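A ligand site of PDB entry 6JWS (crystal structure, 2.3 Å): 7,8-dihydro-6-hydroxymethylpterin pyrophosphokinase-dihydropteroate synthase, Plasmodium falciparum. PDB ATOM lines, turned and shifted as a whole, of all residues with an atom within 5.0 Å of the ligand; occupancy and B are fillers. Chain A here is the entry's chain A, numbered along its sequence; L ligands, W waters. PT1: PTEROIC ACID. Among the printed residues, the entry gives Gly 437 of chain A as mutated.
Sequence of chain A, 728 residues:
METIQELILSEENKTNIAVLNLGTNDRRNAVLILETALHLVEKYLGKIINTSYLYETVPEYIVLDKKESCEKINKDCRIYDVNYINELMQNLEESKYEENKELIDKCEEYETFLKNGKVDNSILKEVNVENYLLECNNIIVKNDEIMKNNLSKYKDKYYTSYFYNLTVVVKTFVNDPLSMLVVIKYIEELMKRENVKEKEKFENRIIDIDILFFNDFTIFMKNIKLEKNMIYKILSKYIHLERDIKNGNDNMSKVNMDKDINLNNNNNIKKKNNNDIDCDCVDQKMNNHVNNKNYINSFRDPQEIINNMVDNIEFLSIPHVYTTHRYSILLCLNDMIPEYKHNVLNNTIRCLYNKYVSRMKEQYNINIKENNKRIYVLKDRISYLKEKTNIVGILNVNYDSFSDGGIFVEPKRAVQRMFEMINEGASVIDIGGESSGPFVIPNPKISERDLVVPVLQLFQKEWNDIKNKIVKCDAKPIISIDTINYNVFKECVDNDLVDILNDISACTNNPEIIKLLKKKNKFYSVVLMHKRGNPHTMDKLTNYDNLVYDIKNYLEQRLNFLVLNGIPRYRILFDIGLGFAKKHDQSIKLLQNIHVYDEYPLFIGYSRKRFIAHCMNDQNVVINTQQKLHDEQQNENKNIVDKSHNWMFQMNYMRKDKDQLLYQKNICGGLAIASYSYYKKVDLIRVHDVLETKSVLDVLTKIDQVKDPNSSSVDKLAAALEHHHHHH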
ATOM      1  N   ASP A 430      16.611  38.657 -35.996  1.00  0.00           N
ATOM      2  CA  ASP A 430      16.308  38.561 -34.574  1.00  0.00           C
ATOM      3  C   ASP A 430      17.481  39.160 -33.816  1.00  0.00           C
ATOM      4  O   ASP A 430      18.568  38.567 -33.769  1.00  0.00           O
ATOM      5  CB  ASP A 430      16.018  37.131 -34.078  1.00  0.00           C
ATOM      6  CG  ASP A 430      15.482  37.052 -32.631  1.00  0.00           C
ATOM      7  OD1 ASP A 430      14.507  37.788 -32.305  1.00  0.00           O
ATOM      8  OD2 ASP A 430      16.044  36.258 -31.816  1.00  0.00           O
ATOM      9  N   SER A 436      20.907  34.018 -23.490  1.00  0.00           N
ATOM     10  CA  SER A 436      20.091  33.081 -22.728  1.00  0.00           C
ATOM     11  C   SER A 436      20.642  31.661 -22.833  1.00  0.00           C
ATOM     12  O   SER A 436      20.092  30.725 -22.232  1.00  0.00           O
ATOM     13  CB  SER A 436      18.629  33.179 -23.146  1.00  0.00           C
ATOM     14  OG  SER A 436      18.488  32.811 -24.513  1.00  0.00           O
ATOM     15  N   GLY A 437      21.765  31.502 -23.554  1.00  0.00           N
ATOM     16  CA  GLY A 437      22.458  30.227 -23.660  1.00  0.00           C
ATOM     17  C   GLY A 437      22.936  29.733 -22.295  1.00  0.00           C
ATOM     18  O   GLY A 437      23.012  30.508 -21.344  1.00  0.00           O
ATOM     19  N   PRO A 438      23.351  28.443 -22.160  1.00  0.00           N
ATOM     20  CA  PRO A 438      23.586  27.851 -20.833  1.00  0.00           C
ATOM     21  C   PRO A 438      24.727  28.501 -20.051  1.00  0.00           C
ATOM     22  O   PRO A 438      25.738  28.914 -20.631  1.00  0.00           O
ATOM     23  CB  PRO A 438      23.911  26.384 -21.166  1.00  0.00           C
ATOM     24  CG  PRO A 438      24.472  26.433 -22.570  1.00  0.00           C
ATOM     25  CD  PRO A 438      23.676  27.523 -23.260  1.00  0.00           C
ATOM     26  N   ASP A 482      14.568  39.884 -29.465  1.00  0.00           N
ATOM     27  CA  ASP A 482      14.638  38.825 -28.477  1.00  0.00           C
ATOM     28  C   ASP A 482      14.813  39.464 -27.093  1.00  0.00           C
ATOM     29  O   ASP A 482      15.929  39.733 -26.639  1.00  0.00           O
ATOM     30  CB  ASP A 482      15.783  37.878 -28.854  1.00  0.00           C
ATOM     31  CG  ASP A 482      15.926  36.634 -27.989  1.00  0.00           C
ATOM     32  OD1 ASP A 482      15.236  36.526 -26.936  1.00  0.00           O
ATOM     33  OD2 ASP A 482      16.726  35.768 -28.385  1.00  0.00           O
ATOM     34  N   ASN A 502      10.090  38.513 -29.796  1.00  0.00           N
ATOM     35  CA  ASN A 502      10.502  37.155 -29.509  1.00  0.00           C
ATOM     36  C   ASN A 502      10.676  37.032 -28.003  1.00  0.00           C
ATOM     37  O   ASN A 502      11.686  37.492 -27.460  1.00  0.00           O
ATOM     38  CB  ASN A 502      11.807  36.820 -30.239  1.00  0.00           C
ATOM     39  CG  ASN A 502      12.336  35.428 -29.971  1.00  0.00           C
ATOM     40  OD1 ASN A 502      11.652  34.576 -29.422  1.00  0.00           O
ATOM     41  ND2 ASN A 502      13.585  35.184 -30.330  1.00  0.00           N
ATOM     42  N   ILE A 504      11.162  34.658 -24.996  1.00  0.00           N
ATOM     43  CA  ILE A 504      11.539  33.289 -24.683  1.00  0.00           C
ATOM     44  C   ILE A 504      10.838  32.805 -23.406  1.00  0.00           C
ATOM     45  O   ILE A 504      10.956  31.636 -23.060  1.00  0.00           O
ATOM     46  CB  ILE A 504      13.065  33.152 -24.570  1.00  0.00           C
ATOM     47  CG1 ILE A 504      13.634  33.995 -23.432  1.00  0.00           C
ATOM     48  CG2 ILE A 504      13.742  33.442 -25.903  1.00  0.00           C
ATOM     49  CD1 ILE A 504      15.053  33.601 -23.085  1.00  0.00           C
ATOM     50  N   VAL A 527       6.548  35.688 -30.882  1.00  0.00           N
ATOM     51  CA  VAL A 527       6.919  34.289 -30.739  1.00  0.00           C
ATOM     52  C   VAL A 527       6.816  33.915 -29.269  1.00  0.00           C
ATOM     53  O   VAL A 527       7.397  34.586 -28.419  1.00  0.00           O
ATOM     54  CB  VAL A 527       8.366  34.079 -31.228  1.00  0.00           C
ATOM     55  CG1 VAL A 527       8.814  32.614 -31.157  1.00  0.00           C
ATOM     56  CG2 VAL A 527       8.576  34.690 -32.626  1.00  0.00           C
ATOM     57  N   MET A 529       7.890  31.039 -26.716  1.00  0.00           N
ATOM     58  CA  MET A 529       8.790  29.913 -26.589  1.00  0.00           C
ATOM     59  C   MET A 529       8.604  29.240 -25.232  1.00  0.00           C
ATOM     60  O   MET A 529       8.318  29.932 -24.251  1.00  0.00           O
ATOM     61  CB  MET A 529      10.250  30.390 -26.692  1.00  0.00           C
ATOM     62  CG  MET A 529      11.189  29.249 -26.997  1.00  0.00           C
ATOM     63  SD  MET A 529      12.922  29.661 -26.692  1.00  0.00           S
ATOM     64  CE  MET A 529      12.967  29.403 -24.913  1.00  0.00           C
ATOM     65  N   MET A 538      18.359  25.960 -15.867  1.00  0.00           N
ATOM     66  CA  MET A 538      17.503  25.287 -16.843  1.00  0.00           C
ATOM     67  C   MET A 538      17.954  23.845 -17.111  1.00  0.00           C
ATOM     68  O   MET A 538      17.095  22.959 -17.199  1.00  0.00           O
ATOM     69  CB  MET A 538      17.345  26.065 -18.153  1.00  0.00           C
ATOM     70  CG  MET A 538      18.565  26.108 -19.012  1.00  0.00           C
ATOM     71  SD  MET A 538      18.204  27.198 -20.406  1.00  0.00           S
ATOM     72  CE  MET A 538      19.725  27.078 -21.333  1.00  0.00           C
ATOM     73  N   ASP A 575       7.114  28.084 -30.304  1.00  0.00           N
ATOM     74  CA  ASP A 575       8.503  27.638 -30.312  1.00  0.00           C
ATOM     75  C   ASP A 575       8.760  26.678 -29.158  1.00  0.00           C
ATOM     76  O   ASP A 575       8.550  27.008 -27.990  1.00  0.00           O
ATOM     77  CB  ASP A 575       9.464  28.831 -30.284  1.00  0.00           C
ATOM     78  CG  ASP A 575      10.936  28.473 -30.452  1.00  0.00           C
ATOM     79  OD1 ASP A 575      11.290  27.244 -30.350  1.00  0.00           O
ATOM     80  OD2 ASP A 575      11.743  29.413 -30.661  1.00  0.00           O
ATOM     81  N   GLY A 577      11.439  25.635 -27.902  1.00  0.00           N
ATOM     82  CA  GLY A 577      12.580  25.978 -27.060  1.00  0.00           C
ATOM     83  C   GLY A 577      13.654  24.888 -26.946  1.00  0.00           C
ATOM     84  O   GLY A 577      14.042  24.514 -25.839  1.00  0.00           O
ATOM     85  N   LEU A 578      14.157  24.400 -28.089  1.00  0.00           N
ATOM     86  CA  LEU A 578      15.258  23.445 -28.121  1.00  0.00           C
ATOM     87  C   LEU A 578      16.394  23.927 -27.223  1.00  0.00           C
ATOM     88  O   LEU A 578      16.728  25.125 -27.228  1.00  0.00           O
ATOM     89  CB  LEU A 578      15.765  23.277 -29.562  1.00  0.00           C
ATOM     90  CG  LEU A 578      14.744  22.674 -30.543  1.00  0.00           C
ATOM     91  CD1 LEU A 578      15.266  22.695 -31.991  1.00  0.00           C
ATOM     92  CD2 LEU A 578      14.345  21.270 -30.131  1.00  0.00           C
ATOM     93  N   GLY A 579      16.965  23.024 -26.422  1.00  0.00           N
ATOM     94  CA  GLY A 579      18.085  23.352 -25.552  1.00  0.00           C
ATOM     95  C   GLY A 579      17.714  24.066 -24.238  1.00  0.00           C
ATOM     96  O   GLY A 579      18.581  24.313 -23.413  1.00  0.00           O
ATOM     97  N   PHE A 580      16.430  24.419 -24.058  1.00  0.00           N
ATOM     98  CA  PHE A 580      16.028  25.187 -22.881  1.00  0.00           C
ATOM     99  C   PHE A 580      15.240  24.291 -21.920  1.00  0.00           C
ATOM    100  O   PHE A 580      14.042  24.092 -22.080  1.00  0.00           O
ATOM    101  CB  PHE A 580      15.061  26.296 -23.278  1.00  0.00           C
ATOM    102  CG  PHE A 580      15.637  27.545 -23.900  1.00  0.00           C
ATOM    103  CD1 PHE A 580      16.054  28.602 -23.096  1.00  0.00           C
ATOM    104  CD2 PHE A 580      15.688  27.698 -25.289  1.00  0.00           C
ATOM    105  CE1 PHE A 580      16.532  29.774 -23.668  1.00  0.00           C
ATOM    106  CE2 PHE A 580      16.185  28.855 -25.865  1.00  0.00           C
ATOM    107  CZ  PHE A 580      16.588  29.901 -25.037  1.00  0.00           C
ATOM    108  N   PHE A 603       8.183  28.219 -35.109  1.00  0.00           N
ATOM    109  CA  PHE A 603       9.480  28.902 -35.085  1.00  0.00           C
ATOM    110  C   PHE A 603      10.382  28.025 -34.219  1.00  0.00           C
ATOM    111  O   PHE A 603       9.993  27.595 -33.133  1.00  0.00           O
ATOM    112  CB  PHE A 603       9.230  30.335 -34.569  1.00  0.00           C
ATOM    113  CG  PHE A 603      10.396  31.291 -34.422  1.00  0.00           C
ATOM    114  CD1 PHE A 603      11.474  31.012 -33.574  1.00  0.00           C
ATOM    115  CD2 PHE A 603      10.405  32.512 -35.097  1.00  0.00           C
ATOM    116  CE1 PHE A 603      12.531  31.907 -33.447  1.00  0.00           C
ATOM    117  CE2 PHE A 603      11.475  33.400 -34.978  1.00  0.00           C
ATOM    118  CZ  PHE A 603      12.535  33.101 -34.155  1.00  0.00           C
ATOM    119  N   ILE A 604      11.554  27.625 -34.744  1.00  0.00           N
ATOM    120  CA  ILE A 604      12.456  26.845 -33.914  1.00  0.00           C
ATOM    121  C   ILE A 604      13.838  27.456 -34.055  1.00  0.00           C
ATOM    122  O   ILE A 604      14.139  28.075 -35.083  1.00  0.00           O
ATOM    123  CB  ILE A 604      12.442  25.354 -34.291  1.00  0.00           C
ATOM    124  CG1 ILE A 604      13.096  25.109 -35.651  1.00  0.00           C
ATOM    125  CG2 ILE A 604      11.035  24.777 -34.183  1.00  0.00           C
ATOM    126  CD1 ILE A 604      13.220  23.640 -36.026  1.00  0.00           C
ATOM    127  N   GLY A 605      14.661  27.256 -33.012  1.00  0.00           N
ATOM    128  CA  GLY A 605      16.059  27.650 -33.010  1.00  0.00           C
ATOM    129  C   GLY A 605      16.966  26.505 -32.545  1.00  0.00           C
ATOM    130  O   GLY A 605      17.008  26.185 -31.362  1.00  0.00           O
ATOM    131  N   ARG A 608      23.670  26.022 -33.653  1.00  0.00           N
ATOM    132  CA  ARG A 608      24.902  25.878 -32.887  1.00  0.00           C
ATOM    133  C   ARG A 608      24.646  25.386 -31.458  1.00  0.00           C
ATOM    134  O   ARG A 608      25.452  25.645 -30.563  1.00  0.00           O
ATOM    135  CB  ARG A 608      25.733  27.174 -32.897  1.00  0.00           C
ATOM    136  CG  ARG A 608      26.282  27.519 -34.272  1.00  0.00           C
ATOM    137  CD  ARG A 608      27.003  28.858 -34.319  1.00  0.00           C
ATOM    138  NE  ARG A 608      27.379  29.277 -35.678  1.00  0.00           N
ATOM    139  CZ  ARG A 608      28.024  30.412 -35.959  1.00  0.00           C
ATOM    140  NH1 ARG A 608      28.363  31.248 -34.968  1.00  0.00           N
ATOM    141  NH2 ARG A 608      28.326  30.726 -37.216  1.00  0.00           N
ATOM    142  N   LYS A 609      23.558  24.644 -31.215  1.00  0.00           N
ATOM    143  CA  LYS A 609      23.262  24.253 -29.844  1.00  0.00           C
ATOM    144  C   LYS A 609      23.924  22.911 -29.521  1.00  0.00           C
ATOM    145  O   LYS A 609      24.164  22.083 -30.399  1.00  0.00           O
ATOM    146  CB  LYS A 609      21.754  24.234 -29.580  1.00  0.00           C
ATOM    147  CG  LYS A 609      21.045  25.582 -29.714  1.00  0.00           C
ATOM    148  CD  LYS A 609      19.620  25.600 -29.219  1.00  0.00           C
ATOM    149  CE  LYS A 609      19.065  26.996 -29.137  1.00  0.00           C
ATOM    150  NZ  LYS A 609      17.605  27.017 -28.876  1.00  0.00           N
ATOM    151  N   ARG A 610      24.192  22.704 -28.229  1.00  0.00           N
ATOM    152  CA  ARG A 610      24.908  21.541 -27.737  1.00  0.00           C
ATOM    153  C   ARG A 610      24.309  20.251 -28.283  1.00  0.00           C
ATOM    154  O   ARG A 610      25.061  19.312 -28.535  1.00  0.00           O
ATOM    155  CB  ARG A 610      24.921  21.516 -26.203  1.00  0.00           C
ATOM    156  CG  ARG A 610      25.707  22.660 -25.560  1.00  0.00           C
ATOM    157  CD  ARG A 610      25.413  22.875 -24.073  1.00  0.00           C
ATOM    158  NE  ARG A 610      23.984  23.098 -23.876  1.00  0.00           N
ATOM    159  CZ  ARG A 610      23.344  23.118 -22.689  1.00  0.00           C
ATOM    160  NH1 ARG A 610      24.007  22.929 -21.554  1.00  0.00           N
ATOM    161  NH2 ARG A 610      22.033  23.336 -22.662  1.00  0.00           N
ATOM    162  N   ARG A 686      15.570  29.850 -36.848  1.00  0.00           N
ATOM    163  CA  ARG A 686      16.419  30.932 -36.343  1.00  0.00           C
ATOM    164  C   ARG A 686      17.872  30.449 -36.357  1.00  0.00           C
ATOM    165  O   ARG A 686      18.236  29.549 -35.610  1.00  0.00           O
ATOM    166  CB  ARG A 686      15.923  31.246 -34.923  1.00  0.00           C
ATOM    167  CG  ARG A 686      16.728  32.306 -34.174  1.00  0.00           C
ATOM    168  CD  ARG A 686      16.234  32.388 -32.722  1.00  0.00           C
ATOM    169  NE  ARG A 686      17.005  33.449 -32.081  1.00  0.00           N
ATOM    170  CZ  ARG A 686      18.170  33.247 -31.464  1.00  0.00           C
ATOM    171  NH1 ARG A 686      18.672  32.031 -31.335  1.00  0.00           N
ATOM    172  NH2 ARG A 686      18.815  34.284 -30.952  1.00  0.00           N
HETATM  173  C2  PT1 L   1      15.334  29.856 -29.495  1.00  0.00           C
HETATM  174  C3  PT1 L   1      16.321  30.756 -28.944  1.00  0.00           C
HETATM  175  C5  PT1 L   1      15.932  32.160 -28.812  1.00  0.00           C
HETATM  176  N6  PT1 L   1      17.567  30.360 -28.554  1.00  0.00           N
HETATM  177  C7  PT1 L   1      13.849  31.672 -29.653  1.00  0.00           C
HETATM  178  N9  PT1 L   1      14.719  32.552 -29.168  1.00  0.00           N
HETATM  179  C10 PT1 L   1      18.434  31.316 -28.055  1.00  0.00           C
HETATM  180  N11 PT1 L   1      12.606  32.127 -29.990  1.00  0.00           N
HETATM  181  C12 PT1 L   1      18.026  32.639 -27.946  1.00  0.00           C
HETATM  182  C21 PT1 L   1      22.381  25.128 -25.946  1.00  0.00           C
HETATM  183  O22 PT1 L   1      23.514  25.033 -26.445  1.00  0.00           O
HETATM  184  O1  PT1 L   1      15.611  28.547 -29.652  1.00  0.00           O
HETATM  185  N4  PT1 L   1      14.130  30.359 -29.797  1.00  0.00           N
HETATM  186  N8  PT1 L   1      16.817  33.040 -28.316  1.00  0.00           N
HETATM  187  C13 PT1 L   1      19.829  30.932 -27.573  1.00  0.00           C
HETATM  188  N14 PT1 L   1      19.661  30.085 -26.354  1.00  0.00           N
HETATM  189  C15 PT1 L   1      20.363  28.894 -26.246  1.00  0.00           C
HETATM  190  C16 PT1 L   1      19.792  27.819 -25.593  1.00  0.00           C
HETATM  191  C17 PT1 L   1      21.667  28.739 -26.787  1.00  0.00           C
HETATM  192  C18 PT1 L   1      20.434  26.572 -25.475  1.00  0.00           C
HETATM  193  C19 PT1 L   1      22.321  27.506 -26.684  1.00  0.00           C
HETATM  194  C20 PT1 L   1      21.697  26.442 -26.046  1.00  0.00           C
HETATM  195  O23 PT1 L   1      21.837  24.146 -25.380  1.00  0.00           O
HETATM  196  O   HOH W   1      21.045  21.799 -26.762  1.00  0.00           O
HETATM  197  O   HOH W   2      14.031  26.504 -30.261  1.00  0.00           O
HETATM  198  O   HOH W   3      21.696  32.542 -29.896  1.00  0.00           O
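NZ of Lys 609 is in hydrogen-bond range of O1 of the ligand. OD1 of Asn 502 sits at hydrogen-bond distance from N11 of the ligand (2.7 Å). OD2 of Asp 575 lies within hydrogen-bond range of N4 of the ligand, at 2.7 Å. The side-chain carboxylate (OD2) of Asp 482 sits at hydrogen-bond distance from a nitrogen (N8) of the ligand. An oxygen (O22) of the ligand lies within hydrogen-bond range of the backbone NH (N) of Arg 610, 3.0 Å away. NE of Arg 610 is in salt-bridge range of O23 of the ligand (2.8 Å). O1 of the ligand sits at hydrogen-bond distance from O of Gly 605 (3.2 Å). NH1 of Arg 686 lies close to N6 of the ligand, at 3.4 Å. OG of Ser 436 lies close to N14 of the ligand (3.5 Å).
The side-chain amino group (NZ) of Lys 609 lies within hydrogen-bond range of the backbone carbonyl oxygen (O) of Gly 605, 2.7 Å away. NZ of Lys 609 is in hydrogen-bond range of O of Leu 578 (2.7 Å). The side-chain amide nitrogen (ND2) of Asn 502 lies within hydrogen-bond range of the side-chain carboxylate (OD2) of Asp 430, 3.1 Å away. The side-chain carboxylate (OD1) of Asp 575 sits at hydrogen-bond distance from the backbone NH (N) of Gly 577, 2.9 Å away. The guanidinium group (NH2) of Arg 686 is in salt-bridge range of the side-chain carboxylate (OD2) of Asp 482, 3.6 Å away. The guanidinium group (NE) of Arg 686 is in salt-bridge range of the side-chain carboxylate (OD2) of Asp 430 (3.0 Å). N of Arg 686 sits at hydrogen-bond distance from O of Ile 604.
The side-chain sulfur (SD) of Met 529 lies close to a nitrogen (N4) of the ligand (3.4 Å). Merely in contact with the ligand: Gly 437 (3.6 Å), Pro 438 (3.6 Å), Ile 504 (3.5 Å), Val 527 (3.997 Å), Gly 579 (3.6 Å), Phe 580 (3.3 Å) and Phe 603 (3.5 Å). Hydrophobic or aromatic side chains that line the ligand: Pro 438, Ile 504, Val 527, Met 529, Phe 580 and Phe 603. 16 residues have an atom within 4 Å of the ligand: Ser 436, Gly 437, Pro 438, Asp 482, Asn 502, Ile 504, Val 527, Met 529, Asp 575, Gly 579, Phe 580, Phe 603, Gly 605, Lys 609, Arg 610 and Arg 686.
Water W2 lies within hydrogen-bond range of an oxygen (O1) of the ligand, the side-chain carboxylate of Asp 575, the backbone NH of Gly 605 and the backbone NH of Leu 578.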
